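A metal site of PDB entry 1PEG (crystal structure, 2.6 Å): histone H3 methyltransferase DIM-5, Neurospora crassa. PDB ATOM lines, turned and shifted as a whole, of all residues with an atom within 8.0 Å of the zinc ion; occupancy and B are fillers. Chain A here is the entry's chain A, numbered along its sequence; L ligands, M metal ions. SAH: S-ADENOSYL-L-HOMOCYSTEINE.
SG of Cys 290 sits close to N6 of the ligand. N of His 226 is in hydrogen-bond range of N7 of the ligand. The backbone carbonyl oxygen (O) of His 226 lies within hydrogen-bond range of a nitrogen (N6) of the ligand.
SG of Cys 297 sits close to N of Gly 299 (3.6 Å). The side-chain sulfur (SG) of Cys 292 sits close to the backbone NH (N) of Thr 294. The side-chain sulfur of Cys 228 lies close to the backbone NH of Arg 298 (3.1 Å). NE2 of His 226 sits close to SG of Cys 228 (3.4 Å).
SG of Cys 297 is bound to the zinc ion, 2.3 Å away. The zinc ion is bound by SG of Cys 292, at 2.3 Å. SG of Cys 290 binds the zinc ion (2.3 Å). SG of Cys 228 binds the zinc ion (2.3 Å).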
ATOM      1  N   HIS A 226      -3.441   8.182   9.587  1.00  0.00           N
ATOM      2  CA  HIS A 226      -3.067   9.583   9.437  1.00  0.00           C
ATOM      3  C   HIS A 226      -4.052  10.500  10.158  1.00  0.00           C
ATOM      4  O   HIS A 226      -5.224  10.188  10.307  1.00  0.00           O
ATOM      5  CB  HIS A 226      -3.036   9.985   7.951  1.00  0.00           C
ATOM      6  CG  HIS A 226      -3.006  11.463   7.734  1.00  0.00           C
ATOM      7  ND1 HIS A 226      -1.869  12.141   7.366  1.00  0.00           N
ATOM      8  CD2 HIS A 226      -3.976  12.398   7.869  1.00  0.00           C
ATOM      9  CE1 HIS A 226      -2.131  13.427   7.284  1.00  0.00           C
ATOM     10  NE2 HIS A 226      -3.404  13.616   7.584  1.00  0.00           N
ATOM     11  N   SER A 227      -3.538  11.641  10.590  1.00  0.00           N
ATOM     12  CA  SER A 227      -4.314  12.631  11.301  1.00  0.00           C
ATOM     13  C   SER A 227      -3.776  13.974  10.885  1.00  0.00           C
ATOM     14  O   SER A 227      -2.695  14.064  10.286  1.00  0.00           O
ATOM     15  CB  SER A 227      -4.157  12.428  12.812  1.00  0.00           C
ATOM     16  OG  SER A 227      -4.619  13.552  13.534  1.00  0.00           O
ATOM     17  N   CYS A 228      -4.518  15.036  11.183  1.00  0.00           N
ATOM     18  CA  CYS A 228      -4.071  16.367  10.807  1.00  0.00           C
ATOM     19  C   CYS A 228      -3.692  17.142  12.071  1.00  0.00           C
ATOM     20  O   CYS A 228      -3.188  18.260  11.999  1.00  0.00           O
ATOM     21  CB  CYS A 228      -5.159  17.060   9.986  1.00  0.00           C
ATOM     22  SG  CYS A 228      -5.265  16.423   8.274  1.00  0.00           S
ATOM     23  N   ASP A 229      -3.931  16.515  13.217  1.00  0.00           N
ATOM     24  CA  ASP A 229      -3.580  17.053  14.528  1.00  0.00           C
ATOM     25  C   ASP A 229      -3.028  15.851  15.270  1.00  0.00           C
ATOM     26  O   ASP A 229      -3.503  15.502  16.361  1.00  0.00           O
ATOM     27  CB  ASP A 229      -4.805  17.602  15.245  1.00  0.00           C
ATOM     28  N   PRO A 230      -2.011  15.182  14.669  1.00  0.00           N
ATOM     29  CA  PRO A 230      -1.354  13.996  15.228  1.00  0.00           C
ATOM     30  C   PRO A 230      -0.922  14.132  16.660  1.00  0.00           C
ATOM     31  O   PRO A 230      -0.820  15.243  17.186  1.00  0.00           O
ATOM     32  CB  PRO A 230      -0.146  13.789  14.304  1.00  0.00           C
ATOM     33  CG  PRO A 230      -0.007  15.059  13.536  1.00  0.00           C
ATOM     34  CD  PRO A 230      -1.391  15.566  13.392  1.00  0.00           C
ATOM     35  N   CYS A 290      -9.501  12.366   3.690  1.00  0.00           N
ATOM     36  CA  CYS A 290      -9.088  12.259   5.095  1.00  0.00           C
ATOM     37  C   CYS A 290     -10.325  12.163   6.011  1.00  0.00           C
ATOM     38  O   CYS A 290     -11.273  12.922   5.870  1.00  0.00           O
ATOM     39  CB  CYS A 290      -8.244  13.474   5.496  1.00  0.00           C
ATOM     40  SG  CYS A 290      -7.255  13.235   7.012  1.00  0.00           S
ATOM     41  N   LEU A 291     -10.290  11.226   6.954  1.00  0.00           N
ATOM     42  CA  LEU A 291     -11.409  11.037   7.862  1.00  0.00           C
ATOM     43  C   LEU A 291     -11.046  11.381   9.304  1.00  0.00           C
ATOM     44  O   LEU A 291     -11.729  10.971  10.244  1.00  0.00           O
ATOM     45  CB  LEU A 291     -11.905   9.593   7.786  1.00  0.00           C
ATOM     46  CG  LEU A 291     -13.139   9.252   6.954  1.00  0.00           C
ATOM     47  CD1 LEU A 291     -14.053   8.344   7.779  1.00  0.00           C
ATOM     48  CD2 LEU A 291     -13.887  10.509   6.522  1.00  0.00           C
ATOM     49  N   CYS A 292      -9.953  12.136   9.451  1.00  0.00           N
ATOM     50  CA  CYS A 292      -9.464  12.541  10.761  1.00  0.00           C
ATOM     51  C   CYS A 292     -10.376  13.615  11.371  1.00  0.00           C
ATOM     52  O   CYS A 292     -10.712  14.596  10.710  1.00  0.00           O
ATOM     53  CB  CYS A 292      -8.065  13.109  10.629  1.00  0.00           C
ATOM     54  SG  CYS A 292      -8.059  14.899  10.285  1.00  0.00           S
ATOM     55  N   GLY A 293     -10.771  13.400  12.622  1.00  0.00           N
ATOM     56  CA  GLY A 293     -11.637  14.366  13.295  1.00  0.00           C
ATOM     57  C   GLY A 293     -10.994  15.744  13.234  1.00  0.00           C
ATOM     58  O   GLY A 293     -11.694  16.736  13.041  1.00  0.00           O
ATOM     59  N   THR A 294      -9.672  15.769  13.366  1.00  0.00           N
ATOM     60  CA  THR A 294      -8.863  17.000  13.336  1.00  0.00           C
ATOM     61  C   THR A 294      -9.492  18.204  12.639  1.00  0.00           C
ATOM     62  O   THR A 294      -9.627  18.241  11.408  1.00  0.00           O
ATOM     63  CB  THR A 294      -7.506  16.709  12.722  1.00  0.00           C
ATOM     64  N   ALA A 295      -9.854  19.192  13.456  1.00  0.00           N
ATOM     65  CA  ALA A 295     -10.453  20.427  12.994  1.00  0.00           C
ATOM     66  C   ALA A 295      -9.510  21.109  12.021  1.00  0.00           C
ATOM     67  O   ALA A 295      -9.939  21.860  11.137  1.00  0.00           O
ATOM     68  CB  ALA A 295     -10.705  21.327  14.187  1.00  0.00           C
ATOM     69  N   LYS A 296      -8.221  20.854  12.174  1.00  0.00           N
ATOM     70  CA  LYS A 296      -7.217  21.477  11.324  1.00  0.00           C
ATOM     71  C   LYS A 296      -6.997  20.681  10.040  1.00  0.00           C
ATOM     72  O   LYS A 296      -6.101  21.010   9.252  1.00  0.00           O
ATOM     73  CB  LYS A 296      -5.890  21.607  12.099  1.00  0.00           C
ATOM     74  N   CYS A 297      -7.832  19.668   9.817  1.00  0.00           N
ATOM     75  CA  CYS A 297      -7.696  18.794   8.638  1.00  0.00           C
ATOM     76  C   CYS A 297      -7.278  19.428   7.319  1.00  0.00           C
ATOM     77  O   CYS A 297      -8.008  20.203   6.726  1.00  0.00           O
ATOM     78  CB  CYS A 297      -8.979  17.999   8.417  1.00  0.00           C
ATOM     79  SG  CYS A 297      -8.712  16.696   7.163  1.00  0.00           S
ATOM     80  N   ARG A 298      -6.091  19.042   6.843  1.00  0.00           N
ATOM     81  CA  ARG A 298      -5.532  19.570   5.598  1.00  0.00           C
ATOM     82  C   ARG A 298      -6.248  19.102   4.318  1.00  0.00           C
ATOM     83  O   ARG A 298      -5.634  19.091   3.252  1.00  0.00           O
ATOM     84  CB  ARG A 298      -4.047  19.236   5.523  1.00  0.00           C
ATOM     85  N   GLY A 299      -7.510  18.715   4.439  1.00  0.00           N
ATOM     86  CA  GLY A 299      -8.252  18.263   3.256  1.00  0.00           C
ATOM     87  C   GLY A 299      -8.169  16.773   2.958  1.00  0.00           C
ATOM     88  O   GLY A 299      -9.168  16.048   3.102  1.00  0.00           O
ATOM     89  N   TYR A 300      -6.997  16.311   2.519  1.00  0.00           N
ATOM     90  CA  TYR A 300      -6.761  14.902   2.188  1.00  0.00           C
ATOM     91  C   TYR A 300      -5.426  14.422   2.797  1.00  0.00           C
ATOM     92  O   TYR A 300      -4.852  15.089   3.663  1.00  0.00           O
ATOM     93  CB  TYR A 300      -6.752  14.735   0.659  1.00  0.00           C
ATOM     94  N   LEU A 301      -4.921  13.259   2.370  1.00  0.00           N
ATOM     95  CA  LEU A 301      -3.641  12.765   2.869  1.00  0.00           C
ATOM     96  C   LEU A 301      -2.619  12.913   1.770  1.00  0.00           C
ATOM     97  O   LEU A 301      -2.977  13.084   0.605  1.00  0.00           O
ATOM     98  CB  LEU A 301      -3.728  11.297   3.270  1.00  0.00           C
ATOM     99  CG  LEU A 301      -5.069  10.706   3.659  1.00  0.00           C
ATOM    100  CD1 LEU A 301      -4.899   9.231   3.907  1.00  0.00           C
ATOM    101  CD2 LEU A 301      -5.586  11.398   4.891  1.00  0.00           C
HETATM  102  N   SAH L   1      -5.542   1.482   8.278  1.00  0.00           N
HETATM  103  CA  SAH L   1      -4.764   0.811   7.262  1.00  0.00           C
HETATM  104  CB  SAH L   1      -3.297   1.175   7.454  1.00  0.00           C
HETATM  105  CG  SAH L   1      -2.954   2.562   6.961  1.00  0.00           C
HETATM  106  SD  SAH L   1      -1.643   2.656   5.702  1.00  0.00           S
HETATM  107  C   SAH L   1      -4.923  -0.716   7.250  1.00  0.00           C
HETATM  108  O   SAH L   1      -4.045  -1.459   6.635  1.00  0.00           O
HETATM  109  OXT SAH L   1      -6.000  -1.240   7.779  1.00  0.00           O
HETATM  110  C5' SAH L   1      -2.258   3.793   4.473  1.00  0.00           C
HETATM  111  C4' SAH L   1      -3.689   3.670   3.999  1.00  0.00           C
HETATM  112  O4' SAH L   1      -4.584   3.699   5.151  1.00  0.00           O
HETATM  113  C3' SAH L   1      -4.158   4.815   3.117  1.00  0.00           C
HETATM  114  O3' SAH L   1      -3.825   4.594   1.754  1.00  0.00           O
HETATM  115  C2' SAH L   1      -5.662   4.805   3.354  1.00  0.00           C
HETATM  116  O2' SAH L   1      -6.325   3.788   2.622  1.00  0.00           O
HETATM  117  C1' SAH L   1      -5.732   4.482   4.853  1.00  0.00           C
HETATM  118  N9  SAH L   1      -5.687   5.683   5.695  1.00  0.00           N
HETATM  119  C8  SAH L   1      -4.882   5.907   6.789  1.00  0.00           C
HETATM  120  N7  SAH L   1      -5.054   7.087   7.341  1.00  0.00           N
HETATM  121  C5  SAH L   1      -6.037   7.681   6.559  1.00  0.00           C
HETATM  122  C6  SAH L   1      -6.666   8.929   6.614  1.00  0.00           C
HETATM  123  N6  SAH L   1      -6.380   9.864   7.538  1.00  0.00           N
HETATM  124  N1  SAH L   1      -7.611   9.206   5.694  1.00  0.00           N
HETATM  125  C2  SAH L   1      -7.898   8.278   4.793  1.00  0.00           C
HETATM  126  N3  SAH L   1      -7.384   7.066   4.623  1.00  0.00           N
HETATM  127  C4  SAH L   1      -6.445   6.822   5.550  1.00  0.00           C
HETATM  128 ZN    ZN M   1      -7.262  15.228   8.160  1.00  0.00          ZN
